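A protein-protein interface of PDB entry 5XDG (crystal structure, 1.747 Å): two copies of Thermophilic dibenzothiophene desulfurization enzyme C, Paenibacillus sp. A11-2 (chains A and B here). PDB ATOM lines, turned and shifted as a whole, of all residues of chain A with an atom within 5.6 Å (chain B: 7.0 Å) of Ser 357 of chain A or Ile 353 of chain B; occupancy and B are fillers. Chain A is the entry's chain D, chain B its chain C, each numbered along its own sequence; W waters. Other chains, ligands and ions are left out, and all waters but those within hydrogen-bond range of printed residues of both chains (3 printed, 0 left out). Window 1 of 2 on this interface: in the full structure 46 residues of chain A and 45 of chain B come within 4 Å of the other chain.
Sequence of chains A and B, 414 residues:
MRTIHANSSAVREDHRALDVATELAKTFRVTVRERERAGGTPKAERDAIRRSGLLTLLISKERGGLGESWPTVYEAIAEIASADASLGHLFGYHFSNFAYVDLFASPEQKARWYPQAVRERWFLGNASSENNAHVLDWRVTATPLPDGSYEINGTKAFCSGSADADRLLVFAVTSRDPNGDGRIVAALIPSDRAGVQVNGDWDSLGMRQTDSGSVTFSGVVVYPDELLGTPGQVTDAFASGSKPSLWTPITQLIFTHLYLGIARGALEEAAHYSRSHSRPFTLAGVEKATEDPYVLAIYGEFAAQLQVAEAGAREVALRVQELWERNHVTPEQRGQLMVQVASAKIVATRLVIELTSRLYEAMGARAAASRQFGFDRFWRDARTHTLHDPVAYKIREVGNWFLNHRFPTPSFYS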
ATOM      1  N   VAL A 352      18.469   5.444  11.376  1.00  0.00           N
ATOM      2  CA  VAL A 352      17.223   4.734  11.111  1.00  0.00           C
ATOM      3  C   VAL A 352      16.078   5.722  10.908  1.00  0.00           C
ATOM      4  O   VAL A 352      15.217   5.523  10.044  1.00  0.00           O
ATOM      5  CB  VAL A 352      16.923   3.710  12.220  1.00  0.00           C
ATOM      6  CG1 VAL A 352      16.595   4.394  13.531  1.00  0.00           C
ATOM      7  CG2 VAL A 352      15.768   2.783  11.782  1.00  0.00           C
ATOM      8  N   ILE A 353      16.069   6.819  11.665  1.00  0.00           N
ATOM      9  CA  ILE A 353      14.976   7.782  11.542  1.00  0.00           C
ATOM     10  C   ILE A 353      14.989   8.441  10.164  1.00  0.00           C
ATOM     11  O   ILE A 353      13.937   8.620   9.529  1.00  0.00           O
ATOM     12  CB  ILE A 353      15.047   8.813  12.686  1.00  0.00           C
ATOM     13  CG1 ILE A 353      14.733   8.124  14.017  1.00  0.00           C
ATOM     14  CG2 ILE A 353      14.025   9.918  12.473  1.00  0.00           C
ATOM     15  CD1 ILE A 353      13.349   7.503  14.040  1.00  0.00           C
ATOM     16  N   GLU A 354      16.172   8.799   9.668  1.00  0.00           N
ATOM     17  CA  GLU A 354      16.233   9.433   8.357  1.00  0.00           C
ATOM     18  C   GLU A 354      15.903   8.438   7.245  1.00  0.00           C
ATOM     19  O   GLU A 354      15.091   8.731   6.362  1.00  0.00           O
ATOM     20  CB  GLU A 354      17.612  10.072   8.138  1.00  0.00           C
ATOM     21  CG  GLU A 354      17.794  10.656   6.721  1.00  0.00           C
ATOM     22  CD  GLU A 354      17.442  12.144   6.594  1.00  0.00           C
ATOM     23  OE1 GLU A 354      17.877  12.773   5.599  1.00  0.00           O
ATOM     24  OE2 GLU A 354      16.733  12.682   7.474  1.00  0.00           O
ATOM     25  N   LEU A 355      16.507   7.241   7.271  1.00  0.00           N
ATOM     26  CA  LEU A 355      16.342   6.371   6.109  1.00  0.00           C
ATOM     27  C   LEU A 355      14.934   5.785   6.029  1.00  0.00           C
ATOM     28  O   LEU A 355      14.397   5.630   4.924  1.00  0.00           O
ATOM     29  CB  LEU A 355      17.417   5.278   6.090  1.00  0.00           C
ATOM     30  CG  LEU A 355      17.425   3.955   6.850  1.00  0.00           C
ATOM     31  CD1 LEU A 355      16.385   2.997   6.322  1.00  0.00           C
ATOM     32  CD2 LEU A 355      18.813   3.326   6.696  1.00  0.00           C
ATOM     33  N   THR A 356      14.298   5.476   7.164  1.00  0.00           N
ATOM     34  CA  THR A 356      12.964   4.882   7.055  1.00  0.00           C
ATOM     35  C   THR A 356      11.943   5.862   6.490  1.00  0.00           C
ATOM     36  O   THR A 356      10.909   5.428   5.973  1.00  0.00           O
ATOM     37  CB  THR A 356      12.481   4.354   8.404  1.00  0.00           C
ATOM     38  OG1 THR A 356      12.412   5.424   9.351  1.00  0.00           O
ATOM     39  CG2 THR A 356      13.433   3.270   8.914  1.00  0.00           C
ATOM     40  N   SER A 357      12.223   7.160   6.543  1.00  0.00           N
ATOM     41  CA  SER A 357      11.375   8.163   5.913  1.00  0.00           C
ATOM     42  C   SER A 357      11.831   8.476   4.484  1.00  0.00           C
ATOM     43  O   SER A 357      11.023   8.448   3.547  1.00  0.00           O
ATOM     44  CB  SER A 357      11.351   9.425   6.788  1.00  0.00           C
ATOM     45  OG  SER A 357      10.651  10.484   6.172  1.00  0.00           O
ATOM     46  N   ARG A 358      13.132   8.710   4.288  1.00  0.00           N
ATOM     47  CA  ARG A 358      13.635   9.189   3.003  1.00  0.00           C
ATOM     48  C   ARG A 358      13.654   8.112   1.919  1.00  0.00           C
ATOM     49  O   ARG A 358      13.653   8.452   0.727  1.00  0.00           O
ATOM     50  CB  ARG A 358      15.044   9.758   3.172  1.00  0.00           C
ATOM     51  CG  ARG A 358      15.150  10.907   4.172  1.00  0.00           C
ATOM     52  CD  ARG A 358      14.872  12.269   3.544  1.00  0.00           C
ATOM     53  NE  ARG A 358      15.301  12.363   2.147  1.00  0.00           N
ATOM     54  CZ  ARG A 358      16.562  12.494   1.746  1.00  0.00           C
ATOM     55  NH1 ARG A 358      17.546  12.537   2.635  1.00  0.00           N
ATOM     56  NH2 ARG A 358      16.839  12.566   0.449  1.00  0.00           N
ATOM     57  N   LEU A 359      13.678   6.827   2.291  1.00  0.00           N
ATOM     58  CA  LEU A 359      13.746   5.786   1.268  1.00  0.00           C
ATOM     59  C   LEU A 359      12.511   5.772   0.369  1.00  0.00           C
ATOM     60  O   LEU A 359      12.570   5.219  -0.734  1.00  0.00           O
ATOM     61  CB  LEU A 359      13.952   4.418   1.907  1.00  0.00           C
ATOM     62  CG  LEU A 359      15.405   4.053   2.163  1.00  0.00           C
ATOM     63  CD1 LEU A 359      15.484   2.796   3.027  1.00  0.00           C
ATOM     64  CD2 LEU A 359      16.129   3.855   0.851  1.00  0.00           C
ATOM     65  N   TYR A 360      11.407   6.399   0.782  1.00  0.00           N
ATOM     66  CA  TYR A 360      10.291   6.536  -0.153  1.00  0.00           C
ATOM     67  C   TYR A 360      10.718   7.266  -1.420  1.00  0.00           C
ATOM     68  O   TYR A 360      10.215   6.978  -2.513  1.00  0.00           O
ATOM     69  CB  TYR A 360       9.118   7.264   0.511  1.00  0.00           C
ATOM     70  CG  TYR A 360       8.252   6.378   1.382  1.00  0.00           C
ATOM     71  CD1 TYR A 360       7.201   5.657   0.833  1.00  0.00           C
ATOM     72  CD2 TYR A 360       8.466   6.283   2.751  1.00  0.00           C
ATOM     73  CE1 TYR A 360       6.396   4.845   1.614  1.00  0.00           C
ATOM     74  CE2 TYR A 360       7.660   5.476   3.552  1.00  0.00           C
ATOM     75  CZ  TYR A 360       6.621   4.763   2.973  1.00  0.00           C
ATOM     76  OH  TYR A 360       5.807   3.963   3.748  1.00  0.00           O
ATOM     77  N   GLU A 361      11.629   8.226  -1.291  1.00  0.00           N
ATOM     78  CA  GLU A 361      12.079   8.986  -2.448  1.00  0.00           C
ATOM     79  C   GLU A 361      12.815   8.112  -3.456  1.00  0.00           C
ATOM     80  O   GLU A 361      12.930   8.495  -4.622  1.00  0.00           O
ATOM     81  CB  GLU A 361      12.940  10.155  -1.966  1.00  0.00           C
ATOM     82  CG  GLU A 361      12.110  11.215  -1.239  1.00  0.00           C
ATOM     83  CD  GLU A 361      12.935  12.106  -0.311  1.00  0.00           C
ATOM     84  OE1 GLU A 361      12.565  12.246   0.890  1.00  0.00           O
ATOM     85  OE2 GLU A 361      13.943  12.673  -0.794  1.00  0.00           O
ATOM     86  N   TRP A 379       9.407   2.975   9.666  1.00  0.00           N
ATOM     87  CA  TRP A 379       9.433   4.273  10.343  1.00  0.00           C
ATOM     88  C   TRP A 379       8.660   4.224  11.661  1.00  0.00           C
ATOM     89  O   TRP A 379       9.131   4.718  12.691  1.00  0.00           O
ATOM     90  CB  TRP A 379       8.867   5.368   9.428  1.00  0.00           C
ATOM     91  CG  TRP A 379       8.762   6.710  10.115  1.00  0.00           C
ATOM     92  CD1 TRP A 379       9.755   7.650  10.247  1.00  0.00           C
ATOM     93  CD2 TRP A 379       7.605   7.257  10.765  1.00  0.00           C
ATOM     94  NE1 TRP A 379       9.284   8.753  10.928  1.00  0.00           N
ATOM     95  CE2 TRP A 379       7.965   8.540  11.254  1.00  0.00           C
ATOM     96  CE3 TRP A 379       6.295   6.802  10.960  1.00  0.00           C
ATOM     97  CZ2 TRP A 379       7.074   9.350  11.944  1.00  0.00           C
ATOM     98  CZ3 TRP A 379       5.402   7.612  11.653  1.00  0.00           C
ATOM     99  CH2 TRP A 379       5.801   8.877  12.133  1.00  0.00           C
ATOM    100  N   ALA B 263       2.894  21.426   7.600  1.00  0.00           N
ATOM    101  CA  ALA B 263       3.991  21.738   8.520  1.00  0.00           C
ATOM    102  C   ALA B 263       3.519  22.609   9.678  1.00  0.00           C
ATOM    103  O   ALA B 263       3.845  22.343  10.843  1.00  0.00           O
ATOM    104  CB  ALA B 263       5.143  22.412   7.768  1.00  0.00           C
ATOM    105  N   PHE B 302      12.584  24.493  13.523  1.00  0.00           N
ATOM    106  CA  PHE B 302      11.528  24.261  12.547  1.00  0.00           C
ATOM    107  C   PHE B 302      10.609  25.473  12.406  1.00  0.00           C
ATOM    108  O   PHE B 302      10.194  25.813  11.291  1.00  0.00           O
ATOM    109  CB  PHE B 302      10.756  22.997  12.938  1.00  0.00           C
ATOM    110  CG  PHE B 302      11.533  21.725  12.683  1.00  0.00           C
ATOM    111  CD1 PHE B 302      12.061  21.471  11.426  1.00  0.00           C
ATOM    112  CD2 PHE B 302      11.794  20.828  13.702  1.00  0.00           C
ATOM    113  CE1 PHE B 302      12.787  20.326  11.176  1.00  0.00           C
ATOM    114  CE2 PHE B 302      12.529  19.676  13.459  1.00  0.00           C
ATOM    115  CZ  PHE B 302      13.031  19.427  12.199  1.00  0.00           C
ATOM    116  N   VAL B 347      12.094  23.553  -0.663  1.00  0.00           N
ATOM    117  CA  VAL B 347      12.291  23.927   0.733  1.00  0.00           C
ATOM    118  C   VAL B 347      11.136  23.416   1.588  1.00  0.00           C
ATOM    119  O   VAL B 347      11.348  22.833   2.657  1.00  0.00           O
ATOM    120  CB  VAL B 347      12.474  25.457   0.850  1.00  0.00           C
ATOM    121  CG1 VAL B 347      12.384  25.918   2.300  1.00  0.00           C
ATOM    122  CG2 VAL B 347      13.832  25.869   0.254  1.00  0.00           C
ATOM    123  N   ALA B 348       9.895  23.593   1.114  1.00  0.00           N
ATOM    124  CA  ALA B 348       8.739  23.115   1.869  1.00  0.00           C
ATOM    125  C   ALA B 348       8.744  21.594   2.009  1.00  0.00           C
ATOM    126  O   ALA B 348       8.343  21.060   3.051  1.00  0.00           O
ATOM    127  CB  ALA B 348       7.446  23.580   1.202  1.00  0.00           C
ATOM    128  N   THR B 349       9.157  20.881   0.960  1.00  0.00           N
ATOM    129  CA  THR B 349       9.226  19.421   1.021  1.00  0.00           C
ATOM    130  C   THR B 349      10.212  18.949   2.089  1.00  0.00           C
ATOM    131  O   THR B 349       9.866  18.136   2.951  1.00  0.00           O
ATOM    132  CB  THR B 349       9.618  18.851  -0.346  1.00  0.00           C
ATOM    133  OG1 THR B 349       8.580  19.107  -1.305  1.00  0.00           O
ATOM    134  CG2 THR B 349       9.856  17.342  -0.255  1.00  0.00           C
ATOM    135  N   ARG B 350      11.464  19.417   2.023  1.00  0.00           N
ATOM    136  CA  ARG B 350      12.432  19.040   3.052  1.00  0.00           C
ATOM    137  C   ARG B 350      11.910  19.377   4.445  1.00  0.00           C
ATOM    138  O   ARG B 350      12.005  18.565   5.374  1.00  0.00           O
ATOM    139  CB  ARG B 350      13.775  19.733   2.811  1.00  0.00           C
ATOM    140  CG  ARG B 350      14.405  19.431   1.456  1.00  0.00           C
ATOM    141  CD  ARG B 350      14.432  17.939   1.175  1.00  0.00           C
ATOM    142  NE  ARG B 350      15.343  17.593   0.086  1.00  0.00           N
ATOM    143  CZ  ARG B 350      15.416  16.387  -0.465  1.00  0.00           C
ATOM    144  NH1 ARG B 350      16.275  16.157  -1.449  1.00  0.00           N
ATOM    145  NH2 ARG B 350      14.622  15.409  -0.038  1.00  0.00           N
ATOM    146  N   LEU B 351      11.333  20.566   4.601  1.00  0.00           N
ATOM    147  CA  LEU B 351      10.883  21.012   5.912  1.00  0.00           C
ATOM    148  C   LEU B 351       9.792  20.098   6.472  1.00  0.00           C
ATOM    149  O   LEU B 351       9.875  19.639   7.619  1.00  0.00           O
ATOM    150  CB  LEU B 351      10.399  22.462   5.818  1.00  0.00           C
ATOM    151  CG  LEU B 351       9.689  23.017   7.049  1.00  0.00           C
ATOM    152  CD1 LEU B 351      10.612  22.935   8.268  1.00  0.00           C
ATOM    153  CD2 LEU B 351       9.277  24.459   6.785  1.00  0.00           C
ATOM    154  N   VAL B 352       8.754  19.820   5.682  1.00  0.00           N
ATOM    155  CA  VAL B 352       7.618  19.105   6.259  1.00  0.00           C
ATOM    156  C   VAL B 352       7.989  17.656   6.533  1.00  0.00           C
ATOM    157  O   VAL B 352       7.517  17.074   7.512  1.00  0.00           O
ATOM    158  CB  VAL B 352       6.361  19.217   5.373  1.00  0.00           C
ATOM    159  CG1 VAL B 352       6.510  18.445   4.063  1.00  0.00           C
ATOM    160  CG2 VAL B 352       5.136  18.739   6.143  1.00  0.00           C
ATOM    161  N   ILE B 353       8.877  17.070   5.719  1.00  0.00           N
ATOM    162  CA  ILE B 353       9.247  15.670   5.939  1.00  0.00           C
ATOM    163  C   ILE B 353      10.129  15.527   7.179  1.00  0.00           C
ATOM    164  O   ILE B 353       9.985  14.566   7.948  1.00  0.00           O
ATOM    165  CB  ILE B 353       9.915  15.079   4.685  1.00  0.00           C
ATOM    166  CG1 ILE B 353       8.885  14.943   3.553  1.00  0.00           C
ATOM    167  CG2 ILE B 353      10.577  13.735   5.012  1.00  0.00           C
ATOM    168  CD1 ILE B 353       7.721  13.967   3.837  1.00  0.00           C
ATOM    169  N   GLU B 354      11.053  16.463   7.401  1.00  0.00           N
ATOM    170  CA  GLU B 354      11.847  16.405   8.634  1.00  0.00           C
ATOM    171  C   GLU B 354      10.994  16.707   9.863  1.00  0.00           C
ATOM    172  O   GLU B 354      11.046  15.988  10.869  1.00  0.00           O
ATOM    173  CB  GLU B 354      13.016  17.388   8.579  1.00  0.00           C
ATOM    174  CG  GLU B 354      13.931  17.250   7.392  1.00  0.00           C
ATOM    175  CD  GLU B 354      15.073  18.245   7.460  1.00  0.00           C
ATOM    176  OE1 GLU B 354      15.964  18.206   6.580  1.00  0.00           O
ATOM    177  OE2 GLU B 354      15.075  19.067   8.406  1.00  0.00           O
ATOM    178  N   LEU B 355      10.210  17.788   9.804  1.00  0.00           N
ATOM    179  CA  LEU B 355       9.476  18.262  10.969  1.00  0.00           C
ATOM    180  C   LEU B 355       8.467  17.225  11.468  1.00  0.00           C
ATOM    181  O   LEU B 355       8.377  16.961  12.673  1.00  0.00           O
ATOM    182  CB  LEU B 355       8.809  19.583  10.579  1.00  0.00           C
ATOM    183  CG  LEU B 355       7.780  20.410  11.306  1.00  0.00           C
ATOM    184  CD1 LEU B 355       7.776  21.765  10.597  1.00  0.00           C
ATOM    185  CD2 LEU B 355       6.432  19.736  11.196  1.00  0.00           C
ATOM    186  N   THR B 356       7.689  16.626  10.561  1.00  0.00           N
ATOM    187  CA  THR B 356       6.634  15.712  10.996  1.00  0.00           C
ATOM    188  C   THR B 356       7.201  14.451  11.637  1.00  0.00           C
ATOM    189  O   THR B 356       6.502  13.779  12.402  1.00  0.00           O
ATOM    190  CB  THR B 356       5.722  15.348   9.818  1.00  0.00           C
ATOM    191  OG1 THR B 356       6.495  14.755   8.771  1.00  0.00           O
ATOM    192  CG2 THR B 356       5.040  16.612   9.284  1.00  0.00           C
ATOM    193  N   SER B 357       8.456  14.128  11.350  1.00  0.00           N
ATOM    194  CA  SER B 357       9.141  13.004  11.982  1.00  0.00           C
ATOM    195  C   SER B 357       9.888  13.417  13.251  1.00  0.00           C
ATOM    196  O   SER B 357       9.740  12.788  14.307  1.00  0.00           O
ATOM    197  CB  SER B 357      10.116  12.384  10.979  1.00  0.00           C
ATOM    198  OG  SER B 357      10.865  11.337  11.564  1.00  0.00           O
ATOM    199  N   ARG B 358      10.689  14.485  13.171  1.00  0.00           N
ATOM    200  CA  ARG B 358      11.572  14.861  14.280  1.00  0.00           C
ATOM    201  C   ARG B 358      10.828  15.463  15.472  1.00  0.00           C
ATOM    202  O   ARG B 358      11.357  15.445  16.590  1.00  0.00           O
ATOM    203  CB  ARG B 358      12.634  15.854  13.804  1.00  0.00           C
ATOM    204  CG  ARG B 358      13.488  15.393  12.610  1.00  0.00           C
ATOM    205  CD  ARG B 358      14.750  14.604  12.980  1.00  0.00           C
ATOM    206  NE  ARG B 358      15.345  14.951  14.275  1.00  0.00           N
ATOM    207  CZ  ARG B 358      16.038  16.057  14.538  1.00  0.00           C
ATOM    208  NH1 ARG B 358      16.216  16.977  13.601  1.00  0.00           N
ATOM    209  NH2 ARG B 358      16.544  16.249  15.756  1.00  0.00           N
ATOM    210  N   PHE B 378       0.321  13.586  10.259  1.00  0.00           N
ATOM    211  CA  PHE B 378       1.021  14.642   9.526  1.00  0.00           C
ATOM    212  C   PHE B 378       2.146  14.067   8.667  1.00  0.00           C
ATOM    213  O   PHE B 378       2.266  14.413   7.486  1.00  0.00           O
ATOM    214  CB  PHE B 378       1.566  15.702  10.488  1.00  0.00           C
ATOM    215  CG  PHE B 378       0.499  16.440  11.263  1.00  0.00           C
ATOM    216  CD1 PHE B 378      -0.204  17.491  10.692  1.00  0.00           C
ATOM    217  CD2 PHE B 378       0.213  16.091  12.571  1.00  0.00           C
ATOM    218  CE1 PHE B 378      -1.173  18.164  11.399  1.00  0.00           C
ATOM    219  CE2 PHE B 378      -0.773  16.766  13.291  1.00  0.00           C
ATOM    220  CZ  PHE B 378      -1.457  17.804  12.702  1.00  0.00           C
ATOM    221  N   TRP B 379       2.980  13.190   9.239  1.00  0.00           N
ATOM    222  CA  TRP B 379       4.015  12.536   8.438  1.00  0.00           C
ATOM    223  C   TRP B 379       3.398  11.680   7.332  1.00  0.00           C
ATOM    224  O   TRP B 379       3.876  11.695   6.185  1.00  0.00           O
ATOM    225  CB  TRP B 379       4.935  11.690   9.327  1.00  0.00           C
ATOM    226  CG  TRP B 379       5.962  10.902   8.543  1.00  0.00           C
ATOM    227  CD1 TRP B 379       7.195  11.333   8.121  1.00  0.00           C
ATOM    228  CD2 TRP B 379       5.826   9.559   8.086  1.00  0.00           C
ATOM    229  NE1 TRP B 379       7.830  10.330   7.418  1.00  0.00           N
ATOM    230  CE2 TRP B 379       7.009   9.233   7.384  1.00  0.00           C
ATOM    231  CE3 TRP B 379       4.813   8.594   8.197  1.00  0.00           C
ATOM    232  CZ2 TRP B 379       7.215   7.982   6.806  1.00  0.00           C
ATOM    233  CZ3 TRP B 379       5.018   7.357   7.621  1.00  0.00           C
ATOM    234  CH2 TRP B 379       6.214   7.061   6.933  1.00  0.00           C
ATOM    235  N   ASP B 381       0.544  12.045   5.739  1.00  0.00           N
ATOM    236  CA  ASP B 381       0.006  12.899   4.683  1.00  0.00           C
ATOM    237  C   ASP B 381       1.136  13.516   3.867  1.00  0.00           C
ATOM    238  O   ASP B 381       1.134  13.456   2.633  1.00  0.00           O
ATOM    239  CB  ASP B 381      -0.878  14.003   5.287  1.00  0.00           C
ATOM    240  CG  ASP B 381      -2.164  13.465   5.873  1.00  0.00           C
ATOM    241  OD1 ASP B 381      -2.581  12.350   5.475  1.00  0.00           O
ATOM    242  OD2 ASP B 381      -2.764  14.154   6.729  1.00  0.00           O
ATOM    243  N   ALA B 382       2.111  14.109   4.556  1.00  0.00           N
ATOM    244  CA  ALA B 382       3.229  14.760   3.880  1.00  0.00           C
ATOM    245  C   ALA B 382       4.075  13.758   3.103  1.00  0.00           C
ATOM    246  O   ALA B 382       4.464  14.018   1.957  1.00  0.00           O
ATOM    247  CB  ALA B 382       4.086  15.508   4.905  1.00  0.00           C
ATOM    248  N   ARG B 383       4.390  12.614   3.714  1.00  0.00           N
ATOM    249  CA  ARG B 383       5.246  11.647   3.035  1.00  0.00           C
ATOM    250  C   ARG B 383       4.575  11.131   1.767  1.00  0.00           C
ATOM    251  O   ARG B 383       5.235  10.922   0.744  1.00  0.00           O
ATOM    252  CB  ARG B 383       5.597  10.492   3.987  1.00  0.00           C
ATOM    253  CG  ARG B 383       6.421   9.357   3.353  1.00  0.00           C
ATOM    254  CD  ARG B 383       7.858   9.771   3.031  1.00  0.00           C
ATOM    255  NE  ARG B 383       7.928  10.687   1.885  1.00  0.00           N
ATOM    256  CZ  ARG B 383       9.048  11.228   1.418  1.00  0.00           C
ATOM    257  NH1 ARG B 383      10.215  10.923   1.967  1.00  0.00           N
ATOM    258  NH2 ARG B 383       9.001  12.075   0.389  1.00  0.00           N
ATOM    259  N   THR B 384       3.260  10.929   1.817  1.00  0.00           N
ATOM    260  CA  THR B 384       2.538  10.488   0.630  1.00  0.00           C
ATOM    261  C   THR B 384       2.552  11.558  -0.459  1.00  0.00           C
ATOM    262  O   THR B 384       2.948  11.284  -1.596  1.00  0.00           O
ATOM    263  CB  THR B 384       1.098  10.094   1.004  1.00  0.00           C
ATOM    264  OG1 THR B 384       1.138   9.000   1.917  1.00  0.00           O
ATOM    265  CG2 THR B 384       0.314   9.635  -0.235  1.00  0.00           C
ATOM    266  N   HIS B 385       2.126  12.786  -0.144  1.00  0.00           N
ATOM    267  CA  HIS B 385       1.943  13.748  -1.232  1.00  0.00           C
ATOM    268  C   HIS B 385       3.276  14.205  -1.829  1.00  0.00           C
ATOM    269  O   HIS B 385       3.371  14.414  -3.044  1.00  0.00           O
ATOM    270  CB  HIS B 385       1.128  14.965  -0.796  1.00  0.00           C
ATOM    271  CG  HIS B 385       0.566  15.716  -1.964  1.00  0.00           C
ATOM    272  ND1 HIS B 385       1.329  16.565  -2.744  1.00  0.00           N
ATOM    273  CD2 HIS B 385      -0.654  15.665  -2.549  1.00  0.00           C
ATOM    274  CE1 HIS B 385       0.588  17.039  -3.728  1.00  0.00           C
ATOM    275  NE2 HIS B 385      -0.617  16.507  -3.636  1.00  0.00           N
ATOM    276  N   THR B 386       4.316  14.362  -1.007  1.00  0.00           N
ATOM    277  CA  THR B 386       5.581  14.890  -1.522  1.00  0.00           C
ATOM    278  C   THR B 386       6.196  14.027  -2.624  1.00  0.00           C
ATOM    279  O   THR B 386       7.113  14.498  -3.312  1.00  0.00           O
ATOM    280  CB  THR B 386       6.590  15.073  -0.374  1.00  0.00           C
ATOM    281  OG1 THR B 386       6.658  13.878   0.408  1.00  0.00           O
ATOM    282  CG2 THR B 386       6.176  16.246   0.521  1.00  0.00           C
ATOM    283  N   LEU B 387       5.726  12.791  -2.812  1.00  0.00           N
ATOM    284  CA  LEU B 387       6.209  11.912  -3.867  1.00  0.00           C
ATOM    285  C   LEU B 387       5.496  12.117  -5.199  1.00  0.00           C
ATOM    286  O   LEU B 387       5.844  11.441  -6.176  1.00  0.00           O
ATOM    287  CB  LEU B 387       6.056  10.454  -3.437  1.00  0.00           C
ATOM    288  CG  LEU B 387       6.714  10.125  -2.099  1.00  0.00           C
ATOM    289  CD1 LEU B 387       6.125   8.837  -1.556  1.00  0.00           C
ATOM    290  CD2 LEU B 387       8.232   9.984  -2.283  1.00  0.00           C
HETATM  291  O   HOH W   1      11.704  12.412   7.803  1.00  0.00           O
HETATM  292  O   HOH W   2      12.864  11.150   9.624  1.00  0.00           O
HETATM  293  O   HOH W   3      10.547  14.172  -1.012  1.00  0.00           O
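OE1 of Glu 361 of chain A is in salt-bridge range of NE of Arg 358 of chain A, 3.0 Å away. The side-chain hydroxyl (OG1) of Thr 386 of chain B is in hydrogen-bond range of the guanidinium group (NH2) of Arg 383 of chain B, 3.0 Å away. The guanidinium group (NH1) of Arg 358 of chain A is in salt-bridge range of the side-chain carboxylate (OE1) of Glu 354 of chain A (3.0 Å).
Among the printed residues, merely in contact across the chains: Ile 353 of chain A with Ser 357 of chain B, Ser 357 of chain A with Ile 353 of chain B, Arg 358 of chain A with Arg 350 of chain B, Arg 358 of chain A with Arg 383 of chain B, Tyr 360 of chain A with Arg 383 of chain B, Tyr 360 of chain A with Leu 387 of chain B, Glu 361 of chain A with Leu 387 of chain B and Trp 379 of chain A with Trp 379 of chain B.
The guanidinium group (NH1) of Arg 383 of chain B lies within salt-bridge range of the side-chain carboxylate (OE1) of Glu 361 of chain A, 2.9 Å away. The indole nitrogen (NE1) of Trp 379 of chain A lies within hydrogen-bond range of the side-chain hydroxyl (OG) of Ser 357 of chain B, at 3.1 Å. NH2 of Arg 350 of chain B lies within salt-bridge range of OE2 of Glu 361 of chain A (2.9 Å). OG of Ser 357 of chain A sits at hydrogen-bond distance from NE1 of Trp 379 of chain B (3.1 Å). The guanidinium group of Arg 383 of chain B sits at hydrogen-bond distance from the backbone carbonyl oxygen of Ser 357 of chain A (3.0 Å).
Glu 354 of chain A touches none of the printed residues of chain B. Of chain B, only Ile 353, Trp 379 and Arg 383 come within 4 Å of Ser 357 of chain A. Of the printed residues of chain B, Arg 358 of chain A touches Arg 350 and Arg 383. Printed residues of chain B within 4 Å of Glu 361 of chain A: Arg 350, Arg 383 and Leu 387. Of the printed residues of chain A, Arg 350 of chain B touches Arg 358 (3.6 Å) and Glu 361 (2.9 Å). Ile 353 of chain B touches just one residue of chain A: Ser 357. Thr 384 of chain B touches none of the printed residues of chain A.
Ile 353 of chain A touches Ser 357 of chain B, and with the chains exchanged Ser 357 of chain A touches Ile 353 of chain B. Ser 357 of chain A touches Trp 379 of chain B, and with the chains exchanged Trp 379 of chain A touches Ser 357 of chain B. Trp 379 of chain A touches its own counterpart, Trp 379 of chain B. Positions printed for both chains: 352, 353, 354, 355, 356, 357, 358 and 379.
Hydrophobic or aromatic side chains of chain B within 4 Å of the printed part of chain A: Ile 353, Trp 379 and Leu 387. Of the 11 printed residues of chain A, 6 touch a printed residue of chain B. Hydrophobic or aromatic side chains of chain A within 4 Å of the printed part of chain B: Ile 353, Tyr 360 and Trp 379.
Water W1 lies within hydrogen-bond range of the side-chain hydroxyl (OG) of Ser 357 of chain A (2.7 Å) and the backbone carbonyl oxygen (O) of Ile 353 of chain B (2.8 Å). Water W2 lies within hydrogen-bond range of O of Ile 353 of chain A (2.7 Å) and OG of Ser 357 of chain B (2.8 Å). Water W3 lies within hydrogen-bond range of NH2 of Arg 383 of chain B (3.0 Å) and OE1 of Glu 361 of chain A (3.4 Å).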
